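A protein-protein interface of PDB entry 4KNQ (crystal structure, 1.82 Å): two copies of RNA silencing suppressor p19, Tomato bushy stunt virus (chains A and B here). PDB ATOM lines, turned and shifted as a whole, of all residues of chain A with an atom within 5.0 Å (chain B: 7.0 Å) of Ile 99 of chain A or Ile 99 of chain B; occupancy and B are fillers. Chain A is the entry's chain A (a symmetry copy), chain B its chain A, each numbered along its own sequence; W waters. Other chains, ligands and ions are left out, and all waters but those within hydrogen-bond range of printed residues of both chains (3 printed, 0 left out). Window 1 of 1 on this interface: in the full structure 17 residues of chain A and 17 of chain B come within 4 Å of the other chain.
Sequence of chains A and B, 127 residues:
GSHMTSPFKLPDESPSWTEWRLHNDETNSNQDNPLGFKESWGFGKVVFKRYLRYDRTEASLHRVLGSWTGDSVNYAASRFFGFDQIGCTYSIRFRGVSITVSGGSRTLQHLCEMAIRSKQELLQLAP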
ATOM      1  N   TYR A  90      -9.667  11.915  27.718  1.00  0.00           N
ATOM      2  CA  TYR A  90     -10.046  11.622  29.101  1.00  0.00           C
ATOM      3  C   TYR A  90      -8.735  11.425  29.892  1.00  0.00           C
ATOM      4  O   TYR A  90      -7.838  10.690  29.427  1.00  0.00           O
ATOM      5  CB  TYR A  90     -10.879  10.361  29.182  1.00  0.00           C
ATOM      6  CG  TYR A  90     -11.173   9.979  30.589  1.00  0.00           C
ATOM      7  CD1 TYR A  90     -12.093  10.717  31.380  1.00  0.00           C
ATOM      8  CD2 TYR A  90     -10.497   8.939  31.225  1.00  0.00           C
ATOM      9  CE1 TYR A  90     -12.298  10.421  32.702  1.00  0.00           C
ATOM     10  CE2 TYR A  90     -10.758   8.621  32.524  1.00  0.00           C
ATOM     11  CZ  TYR A  90     -11.655   9.361  33.281  1.00  0.00           C
ATOM     12  OH  TYR A  90     -11.955   9.051  34.578  1.00  0.00           O
ATOM     13  N   SER A  91      -8.616  12.033  31.032  1.00  0.00           N
ATOM     14  CA  SER A  91      -7.488  11.751  31.938  1.00  0.00           C
ATOM     15  C   SER A  91      -7.960  11.468  33.327  1.00  0.00           C
ATOM     16  O   SER A  91      -8.946  12.092  33.842  1.00  0.00           O
ATOM     17  CB  SER A  91      -6.639  13.023  31.884  1.00  0.00           C
ATOM     18  OG  SER A  91      -5.395  12.774  32.503  1.00  0.00           O
ATOM     19  N   ILE A  92      -7.271  10.592  34.038  1.00  0.00           N
ATOM     20  CA  ILE A  92      -7.556  10.329  35.440  1.00  0.00           C
ATOM     21  C   ILE A  92      -6.200  10.131  36.173  1.00  0.00           C
ATOM     22  O   ILE A  92      -5.244   9.615  35.564  1.00  0.00           O
ATOM     23  CB  ILE A  92      -8.488   9.065  35.619  1.00  0.00           C
ATOM     24  CG1 ILE A  92      -8.761   8.794  37.092  1.00  0.00           C
ATOM     25  CG2 ILE A  92      -7.943   7.827  34.910  1.00  0.00           C
ATOM     26  CD1 ILE A  92      -9.923   7.749  37.237  1.00  0.00           C
ATOM     27  N   VAL A  97      -0.450   7.694  39.730  1.00  0.00           N
ATOM     28  CA  VAL A  97      -0.477   7.179  38.355  1.00  0.00           C
ATOM     29  C   VAL A  97      -1.556   7.975  37.593  1.00  0.00           C
ATOM     30  O   VAL A  97      -2.703   8.108  38.082  1.00  0.00           O
ATOM     31  CB  VAL A  97      -0.855   5.688  38.293  1.00  0.00           C
ATOM     32  CG1 VAL A  97      -1.030   5.175  36.882  1.00  0.00           C
ATOM     33  CG2 VAL A  97       0.224   4.860  39.025  1.00  0.00           C
ATOM     34  N   SER A  98      -1.195   8.473  36.426  1.00  0.00           N
ATOM     35  CA  SER A  98      -2.133   9.101  35.495  1.00  0.00           C
ATOM     36  C   SER A  98      -2.349   8.249  34.265  1.00  0.00           C
ATOM     37  O   SER A  98      -1.370   7.696  33.685  1.00  0.00           O
ATOM     38  CB  SER A  98      -1.595  10.493  35.056  1.00  0.00           C
ATOM     39  OG  SER A  98      -2.145  10.770  33.833  1.00  0.00           O
ATOM     40  N   ILE A  99      -3.580   8.178  33.790  1.00  0.00           N
ATOM     41  CA  ILE A  99      -3.955   7.477  32.553  1.00  0.00           C
ATOM     42  C   ILE A  99      -4.662   8.476  31.687  1.00  0.00           C
ATOM     43  O   ILE A  99      -5.565   9.159  32.217  1.00  0.00           O
ATOM     44  CB  ILE A  99      -4.831   6.259  32.780  1.00  0.00           C
ATOM     45  CG1 ILE A  99      -4.144   5.285  33.735  1.00  0.00           C
ATOM     46  CG2 ILE A  99      -5.163   5.564  31.440  1.00  0.00           C
ATOM     47  CD1 ILE A  99      -4.861   3.988  34.020  1.00  0.00           C
ATOM     48  N   THR A 100      -4.298   8.573  30.431  1.00  0.00           N
ATOM     49  CA  THR A 100      -4.971   9.418  29.504  1.00  0.00           C
ATOM     50  C   THR A 100      -5.423   8.568  28.307  1.00  0.00           C
ATOM     51  O   THR A 100      -4.635   7.669  27.833  1.00  0.00           O
ATOM     52  CB  THR A 100      -4.065  10.550  29.011  1.00  0.00           C
ATOM     53  OG1 THR A 100      -3.685  11.409  30.124  1.00  0.00           O
ATOM     54  CG2 THR A 100      -4.817  11.416  28.069  1.00  0.00           C
ATOM     55  N   VAL A 101      -6.640   8.779  27.836  1.00  0.00           N
ATOM     56  CA  VAL A 101      -7.159   8.053  26.701  1.00  0.00           C
ATOM     57  C   VAL A 101      -7.559   9.113  25.714  1.00  0.00           C
ATOM     58  O   VAL A 101      -8.398   9.995  26.056  1.00  0.00           O
ATOM     59  CB  VAL A 101      -8.371   7.202  27.114  1.00  0.00           C
ATOM     60  CG1 VAL A 101      -8.999   6.553  25.857  1.00  0.00           C
ATOM     61  CG2 VAL A 101      -8.042   6.219  28.266  1.00  0.00           C
ATOM     62  N   MET A 114     -12.731   2.627  26.478  1.00  0.00           N
ATOM     63  CA  MET A 114     -11.400   2.472  27.104  1.00  0.00           C
ATOM     64  C   MET A 114     -11.292   3.335  28.349  1.00  0.00           C
ATOM     65  O   MET A 114     -10.605   2.942  29.318  1.00  0.00           O
ATOM     66  CB  MET A 114     -10.282   2.779  26.127  1.00  0.00           C
ATOM     67  CG  MET A 114     -10.170   1.808  24.955  1.00  0.00           C
ATOM     68  SD  MET A 114      -9.918   0.132  25.526  1.00  0.00           S
ATOM     69  CE  MET A 114      -8.690   0.322  26.772  1.00  0.00           C
ATOM     70  N   SER A 118     -10.374   1.998  32.034  1.00  0.00           N
ATOM     71  CA  SER A 118      -9.198   2.498  32.656  1.00  0.00           C
ATOM     72  C   SER A 118      -9.465   3.035  34.055  1.00  0.00           C
ATOM     73  O   SER A 118      -8.749   2.762  35.021  1.00  0.00           O
ATOM     74  CB  SER A 118      -8.507   3.553  31.813  1.00  0.00           C
ATOM     75  OG  SER A 118      -8.115   3.077  30.519  1.00  0.00           O
ATOM     76  N   LEU A 122      -7.800   1.515  37.431  1.00  0.00           N
ATOM     77  CA  LEU A 122      -6.915   2.329  38.236  1.00  0.00           C
ATOM     78  C   LEU A 122      -7.495   2.465  39.664  1.00  0.00           C
ATOM     79  O   LEU A 122      -6.714   2.523  40.648  1.00  0.00           O
ATOM     80  CB  LEU A 122      -6.754   3.718  37.657  1.00  0.00           C
ATOM     81  CG  LEU A 122      -5.833   4.696  38.345  1.00  0.00           C
ATOM     82  CD1 LEU A 122      -4.370   4.146  38.486  1.00  0.00           C
ATOM     83  CD2 LEU A 122      -5.872   6.062  37.670  1.00  0.00           C
ATOM     84  N   THR B  89       6.715   6.972  31.300  1.00  0.00           N
ATOM     85  CA  THR B  89       5.522   6.957  30.529  1.00  0.00           C
ATOM     86  C   THR B  89       5.474   5.801  29.575  1.00  0.00           C
ATOM     87  O   THR B  89       6.416   5.593  28.811  1.00  0.00           O
ATOM     88  CB  THR B  89       5.366   8.225  29.690  1.00  0.00           C
ATOM     89  OG1 THR B  89       5.452   9.368  30.538  1.00  0.00           O
ATOM     90  CG2 THR B  89       4.040   8.271  28.982  1.00  0.00           C
ATOM     91  N   TYR B  90       4.378   5.069  29.579  1.00  0.00           N
ATOM     92  CA  TYR B  90       4.060   4.039  28.588  1.00  0.00           C
ATOM     93  C   TYR B  90       2.949   4.615  27.685  1.00  0.00           C
ATOM     94  O   TYR B  90       1.955   5.168  28.204  1.00  0.00           O
ATOM     95  CB  TYR B  90       3.563   2.775  29.257  1.00  0.00           C
ATOM     96  CG  TYR B  90       3.120   1.760  28.265  1.00  0.00           C
ATOM     97  CD1 TYR B  90       4.055   1.049  27.466  1.00  0.00           C
ATOM     98  CD2 TYR B  90       1.771   1.522  28.009  1.00  0.00           C
ATOM     99  CE1 TYR B  90       3.646   0.178  26.490  1.00  0.00           C
ATOM    100  CE2 TYR B  90       1.384   0.607  27.075  1.00  0.00           C
ATOM    101  CZ  TYR B  90       2.314  -0.070  26.299  1.00  0.00           C
ATOM    102  OH  TYR B  90       1.955  -1.009  25.373  1.00  0.00           O
ATOM    103  N   SER B  91       3.086   4.493  26.401  1.00  0.00           N
ATOM    104  CA  SER B  91       1.991   4.839  25.476  1.00  0.00           C
ATOM    105  C   SER B  91       1.735   3.740  24.497  1.00  0.00           C
ATOM    106  O   SER B  91       2.683   3.045  24.003  1.00  0.00           O
ATOM    107  CB  SER B  91       2.481   6.109  24.775  1.00  0.00           C
ATOM    108  OG  SER B  91       1.410   6.684  24.060  1.00  0.00           O
ATOM    109  N   ILE B  92       0.488   3.556  24.101  1.00  0.00           N
ATOM    110  CA  ILE B  92       0.133   2.604  23.060  1.00  0.00           C
ATOM    111  C   ILE B  92      -0.993   3.239  22.197  1.00  0.00           C
ATOM    112  O   ILE B  92      -1.819   4.002  22.733  1.00  0.00           O
ATOM    113  CB  ILE B  92      -0.330   1.220  23.667  1.00  0.00           C
ATOM    114  CG1 ILE B  92      -0.715   0.244  22.564  1.00  0.00           C
ATOM    115  CG2 ILE B  92      -1.446   1.374  24.697  1.00  0.00           C
ATOM    116  CD1 ILE B  92      -0.864  -1.202  23.159  1.00  0.00           C
ATOM    117  N   ARG B  93      -0.940   2.977  20.906  1.00  0.00           N
ATOM    118  CA  ARG B  93      -1.966   3.416  19.935  1.00  0.00           C
ATOM    119  C   ARG B  93      -2.396   2.266  19.078  1.00  0.00           C
ATOM    120  O   ARG B  93      -1.544   1.502  18.542  1.00  0.00           O
ATOM    121  CB  ARG B  93      -1.399   4.489  19.122  1.00  0.00           C
ATOM    122  CG  ARG B  93      -2.522   5.075  18.232  1.00  0.00           C
ATOM    123  CD  ARG B  93      -2.004   6.238  17.505  1.00  0.00           C
ATOM    124  NE  ARG B  93      -3.045   6.616  16.573  1.00  0.00           N
ATOM    125  CZ  ARG B  93      -3.722   7.747  16.597  1.00  0.00           C
ATOM    126  NH1 ARG B  93      -3.497   8.645  17.542  1.00  0.00           N
ATOM    127  NH2 ARG B  93      -4.654   7.966  15.690  1.00  0.00           N
ATOM    128  N   PHE B  94      -3.713   2.034  19.004  1.00  0.00           N
ATOM    129  CA  PHE B  94      -4.240   0.992  18.138  1.00  0.00           C
ATOM    130  C   PHE B  94      -5.635   1.413  17.697  1.00  0.00           C
ATOM    131  O   PHE B  94      -6.451   1.827  18.498  1.00  0.00           O
ATOM    132  CB  PHE B  94      -4.329  -0.326  18.873  1.00  0.00           C
ATOM    133  CG  PHE B  94      -4.813  -1.477  18.032  1.00  0.00           C
ATOM    134  CD1 PHE B  94      -4.122  -1.866  16.882  1.00  0.00           C
ATOM    135  CD2 PHE B  94      -5.950  -2.243  18.446  1.00  0.00           C
ATOM    136  CE1 PHE B  94      -4.556  -2.957  16.134  1.00  0.00           C
ATOM    137  CE2 PHE B  94      -6.334  -3.316  17.684  1.00  0.00           C
ATOM    138  CZ  PHE B  94      -5.640  -3.676  16.534  1.00  0.00           C
ATOM    139  N   VAL B  97      -7.101   4.998  18.841  1.00  0.00           N
ATOM    140  CA  VAL B  97      -7.167   5.335  20.269  1.00  0.00           C
ATOM    141  C   VAL B  97      -5.738   5.203  20.834  1.00  0.00           C
ATOM    142  O   VAL B  97      -5.066   4.168  20.612  1.00  0.00           O
ATOM    143  CB  VAL B  97      -8.079   4.377  21.057  1.00  0.00           C
ATOM    144  CG1 VAL B  97      -8.048   4.617  22.549  1.00  0.00           C
ATOM    145  CG2 VAL B  97      -9.525   4.507  20.533  1.00  0.00           C
ATOM    146  N   SER B  98      -5.300   6.221  21.551  1.00  0.00           N
ATOM    147  CA  SER B  98      -4.047   6.193  22.304  1.00  0.00           C
ATOM    148  C   SER B  98      -4.294   6.165  23.795  1.00  0.00           C
ATOM    149  O   SER B  98      -5.169   6.916  24.316  1.00  0.00           O
ATOM    150  CB  SER B  98      -3.191   7.446  21.957  1.00  0.00           C
ATOM    151  OG  SER B  98      -2.370   7.682  23.028  1.00  0.00           O
ATOM    152  N   ILE B  99      -3.509   5.389  24.521  1.00  0.00           N
ATOM    153  CA  ILE B  99      -3.544   5.312  25.989  1.00  0.00           C
ATOM    154  C   ILE B  99      -2.156   5.607  26.471  1.00  0.00           C
ATOM    155  O   ILE B  99      -1.213   4.998  25.920  1.00  0.00           O
ATOM    156  CB  ILE B  99      -4.016   3.972  26.522  1.00  0.00           C
ATOM    157  CG1 ILE B  99      -5.394   3.633  25.956  1.00  0.00           C
ATOM    158  CG2 ILE B  99      -4.048   3.976  28.067  1.00  0.00           C
ATOM    159  CD1 ILE B  99      -6.034   2.355  26.436  1.00  0.00           C
ATOM    160  N   THR B 100      -2.009   6.478  27.440  1.00  0.00           N
ATOM    161  CA  THR B 100      -0.745   6.755  28.033  1.00  0.00           C
ATOM    162  C   THR B 100      -0.859   6.532  29.549  1.00  0.00           C
ATOM    163  O   THR B 100      -1.911   6.928  30.172  1.00  0.00           O
ATOM    164  CB  THR B 100      -0.296   8.194  27.764  1.00  0.00           C
ATOM    165  OG1 THR B 100      -0.115   8.403  26.334  1.00  0.00           O
ATOM    166  CG2 THR B 100       1.034   8.426  28.380  1.00  0.00           C
ATOM    167  N   VAL B 101       0.135   5.896  30.146  1.00  0.00           N
ATOM    168  CA  VAL B 101       0.143   5.652  31.569  1.00  0.00           C
ATOM    169  C   VAL B 101       1.424   6.264  32.060  1.00  0.00           C
ATOM    170  O   VAL B 101       2.524   5.878  31.572  1.00  0.00           O
ATOM    171  CB  VAL B 101       0.111   4.142  31.857  1.00  0.00           C
ATOM    172  CG1 VAL B 101       0.271   3.902  33.378  1.00  0.00           C
ATOM    173  CG2 VAL B 101      -1.107   3.439  31.205  1.00  0.00           C
ATOM    174  N   SER B 102       1.350   7.183  32.994  1.00  0.00           N
ATOM    175  CA  SER B 102       2.515   7.998  33.353  1.00  0.00           C
ATOM    176  C   SER B 102       2.579   8.329  34.846  1.00  0.00           C
ATOM    177  O   SER B 102       1.542   8.360  35.515  1.00  0.00           O
ATOM    178  CB  SER B 102       2.561   9.303  32.481  1.00  0.00           C
ATOM    179  OG  SER B 102       1.409  10.061  32.716  1.00  0.00           O
ATOM    180  N   MET B 114      -0.685  -1.071  35.398  1.00  0.00           N
ATOM    181  CA  MET B 114      -1.739  -0.388  34.616  1.00  0.00           C
ATOM    182  C   MET B 114      -1.422  -0.445  33.131  1.00  0.00           C
ATOM    183  O   MET B 114      -2.354  -0.519  32.301  1.00  0.00           O
ATOM    184  CB  MET B 114      -1.942   1.041  35.077  1.00  0.00           C
ATOM    185  CG  MET B 114      -2.489   1.187  36.494  1.00  0.00           C
ATOM    186  SD  MET B 114      -4.061   0.354  36.668  1.00  0.00           S
ATOM    187  CE  MET B 114      -4.929   0.849  35.219  1.00  0.00           C
ATOM    188  N   ALA B 115      -0.131  -0.385  32.771  1.00  0.00           N
ATOM    189  CA  ALA B 115       0.255  -0.373  31.356  1.00  0.00           C
ATOM    190  C   ALA B 115      -0.137  -1.691  30.705  1.00  0.00           C
ATOM    191  O   ALA B 115      -0.727  -1.701  29.642  1.00  0.00           O
ATOM    192  CB  ALA B 115       1.749  -0.108  31.195  1.00  0.00           C
ATOM    193  N   ARG B 117      -2.399  -3.900  31.633  1.00  0.00           N
ATOM    194  CA  ARG B 117      -3.872  -3.994  31.598  1.00  0.00           C
ATOM    195  C   ARG B 117      -4.435  -3.142  30.509  1.00  0.00           C
ATOM    196  O   ARG B 117      -5.280  -3.591  29.762  1.00  0.00           O
ATOM    197  CB  ARG B 117      -4.458  -3.548  32.925  1.00  0.00           C
ATOM    198  CG  ARG B 117      -4.212  -4.502  34.034  1.00  0.00           C
ATOM    199  CD  ARG B 117      -4.653  -3.822  35.350  1.00  0.00           C
ATOM    200  NE  ARG B 117      -5.173  -4.770  36.304  1.00  0.00           N
ATOM    201  CZ  ARG B 117      -4.457  -5.521  37.126  1.00  0.00           C
ATOM    202  NH1 ARG B 117      -3.126  -5.411  37.206  1.00  0.00           N
ATOM    203  NH2 ARG B 117      -5.100  -6.375  37.911  1.00  0.00           N
ATOM    204  N   SER B 118      -3.842  -1.959  30.293  1.00  0.00           N
ATOM    205  CA  SER B 118      -4.297  -1.091  29.265  1.00  0.00           C
ATOM    206  C   SER B 118      -4.044  -1.656  27.874  1.00  0.00           C
ATOM    207  O   SER B 118      -4.901  -1.650  26.987  1.00  0.00           O
ATOM    208  CB  SER B 118      -3.700   0.299  29.382  1.00  0.00           C
ATOM    209  OG  SER B 118      -4.003   0.943  30.626  1.00  0.00           O
ATOM    210  N   LYS B 119      -2.865  -2.232  27.698  1.00  0.00           N
ATOM    211  CA  LYS B 119      -2.504  -2.812  26.452  1.00  0.00           C
ATOM    212  C   LYS B 119      -3.441  -3.968  26.129  1.00  0.00           C
ATOM    213  O   LYS B 119      -3.979  -4.095  25.050  1.00  0.00           O
ATOM    214  CB  LYS B 119      -0.998  -3.257  26.611  1.00  0.00           C
ATOM    215  CG  LYS B 119      -0.554  -4.121  25.431  1.00  0.00           C
ATOM    216  CD  LYS B 119       0.971  -4.330  25.652  1.00  0.00           C
ATOM    217  CE  LYS B 119       1.570  -5.014  24.513  1.00  0.00           C
ATOM    218  NZ  LYS B 119       3.064  -5.153  24.678  1.00  0.00           N
ATOM    219  N   GLU B 121      -6.495  -4.582  27.243  1.00  0.00           N
ATOM    220  CA  GLU B 121      -7.864  -4.061  26.908  1.00  0.00           C
ATOM    221  C   GLU B 121      -7.971  -3.390  25.569  1.00  0.00           C
ATOM    222  O   GLU B 121      -8.884  -3.674  24.817  1.00  0.00           O
ATOM    223  CB  GLU B 121      -8.320  -3.158  28.006  1.00  0.00           C
ATOM    224  CG  GLU B 121      -8.324  -3.924  29.323  1.00  0.00           C
ATOM    225  CD  GLU B 121      -9.743  -4.156  29.890  1.00  0.00           C
ATOM    226  OE1 GLU B 121     -10.614  -4.876  29.229  1.00  0.00           O
ATOM    227  OE2 GLU B 121      -9.954  -3.547  30.989  1.00  0.00           O
ATOM    228  N   LEU B 122      -6.978  -2.545  25.213  1.00  0.00           N
ATOM    229  CA  LEU B 122      -7.061  -1.834  23.955  1.00  0.00           C
ATOM    230  C   LEU B 122      -6.937  -2.838  22.785  1.00  0.00           C
ATOM    231  O   LEU B 122      -7.582  -2.637  21.724  1.00  0.00           O
ATOM    232  CB  LEU B 122      -5.951  -0.812  23.819  1.00  0.00           C
ATOM    233  CG  LEU B 122      -5.901   0.054  22.584  1.00  0.00           C
ATOM    234  CD1 LEU B 122      -7.225   0.865  22.365  1.00  0.00           C
ATOM    235  CD2 LEU B 122      -4.669   0.951  22.587  1.00  0.00           C
HETATM  236  O   HOH W   1      -3.481   9.271  25.398  1.00  0.00           O
HETATM  237  O   HOH W   2      -6.443   1.282  30.788  1.00  0.00           O
HETATM  238  O   HOH W   3      -0.803   9.621  31.333  1.00  0.00           O
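N of Thr 100 of chain A sits at hydrogen-bond distance from O of Thr 100 of chain B, at 2.9 Å.
N of Ser 102 of chain B lies within hydrogen-bond range of O of Ser 98 of chain A (2.9 Å).
OG of Ser 118 of chain B lies within hydrogen-bond range of O of Met 114 of chain B.
O of Tyr 90 of chain A sits at hydrogen-bond distance from N of Val 101 of chain A (2.8 Å).
OG of Ser 118 of chain A sits at hydrogen-bond distance from O of Met 114 of chain A.
N of Val 101 of chain B sits at hydrogen-bond distance from O of Tyr 90 of chain B.
N of Ile 99 of chain B sits at hydrogen-bond distance from O of Ile 92 of chain B (2.8 Å).
The side-chain hydroxyl of Thr 100 of chain B sits at hydrogen-bond distance from the side-chain hydroxyl of Ser 91 of chain B (3.2 Å).
CG1 of Val 101 of chain B touches CG1 of Val 97 of chain A, 3.9 Å away.
Val 97 of chain A touches Ser 102 of chain B (CA to O, 3.7 Å).
Thr 100 of chain B touches Ser 98 of chain A.
Ser 98 of chain A touches Val 101 of chain B.
Met 114 of chain B touches Ile 99 of chain A (CE to CD1, 3.4 Å).
Ser 98 of chain B touches Thr 100 of chain A (O to O, 3.6 Å).
CA of Ile 99 of chain B touches O of Thr 100 of chain A, at 3.2 Å.
Val 101 of chain A touches Ser 98 of chain B.
CE of Met 114 of chain A touches CD1 of Ile 99 of chain B, at 3.4 Å.
Leu 122 of chain B touches Met 114 of chain A (N to CE, 3.7 Å).
Ile 92 of chain A touches none of the printed residues of chain B.
Of the printed residues of chain B, Val 97 of chain A touches Val 101 and Ser 102.
Ile 99 of chain A touches three residues of chain B.
Of the printed residues of chain B, Thr 100 of chain A touches Ser 98 (3.6 Å), Ile 99 (3.2 Å) and Thr 100 (2.9 Å).
Of the printed residues of chain B, Leu 122 of chain A touches Met 114 (3.7 Å).
Thr 89 of chain B touches none of the printed residues of chain A.
Of the printed residues of chain A, Val 97 of chain B touches Val 101 (3.9 Å).
Of chain A, only Ile 99, Thr 100 and Met 114 come within 4 Å of Ile 99 of chain B.
Of the printed residues of chain A, Glu 121 of chain B touches Met 114 (3.7 Å).
The nearest residue of chain B that does not touch Ile 99 of chain A is Val 101 of chain B (4.4 Å).
Printed residues of chain B that touch a printed residue of chain A: Val 97, Ser 98, Ile 99, Thr 100, Val 101, Ser 102, Met 114, Glu 121 and Leu 122.
Printed residues of chain A that touch a printed residue of chain B: Val 97, Ser 98, Ile 99, Thr 100, Val 101, Met 114 and Leu 122.
Along chain A the printed residues that touch a printed residue of chain B span positions 97 to 122.
Ile 99 of chain A touches Thr 100 of chain B, and with the chains exchanged Thr 100 of chain A touches Ile 99 of chain B.
Ile 99 of chain A touches Met 114 of chain B, and with the chains exchanged Met 114 of chain A touches Ile 99 of chain B.
Thr 100 of chain A touches its own counterpart, Thr 100 of chain B.
Met 114 of chain A touches Leu 122 of chain B, and with the chains exchanged Leu 122 of chain A touches Met 114 of chain B.
Of the 17 pairs that touch across the chains among the printed residues, 14 have their exchanged pair printed and touching as well.
Water W2 bridges the side-chain hydroxyl (OG) of Ser 118 of chain A (2.5 Å) and the side-chain hydroxyl (OG) of Ser 118 of chain B (2.5 Å).
Water W3 lies within hydrogen-bond range of the side-chain hydroxyl (OG) of Ser 102 of chain B (2.6 Å), the side-chain hydroxyl (OG) of Ser 98 of chain A (3.1 Å) and the backbone carbonyl oxygen (O) of Thr 100 of chain B (3.1 Å).
Water W1 bridges the side-chain hydroxyl of Ser 98 of chain B (3.1 Å) and the backbone carbonyl oxygen of Thr 100 of chain A (3.1 Å).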
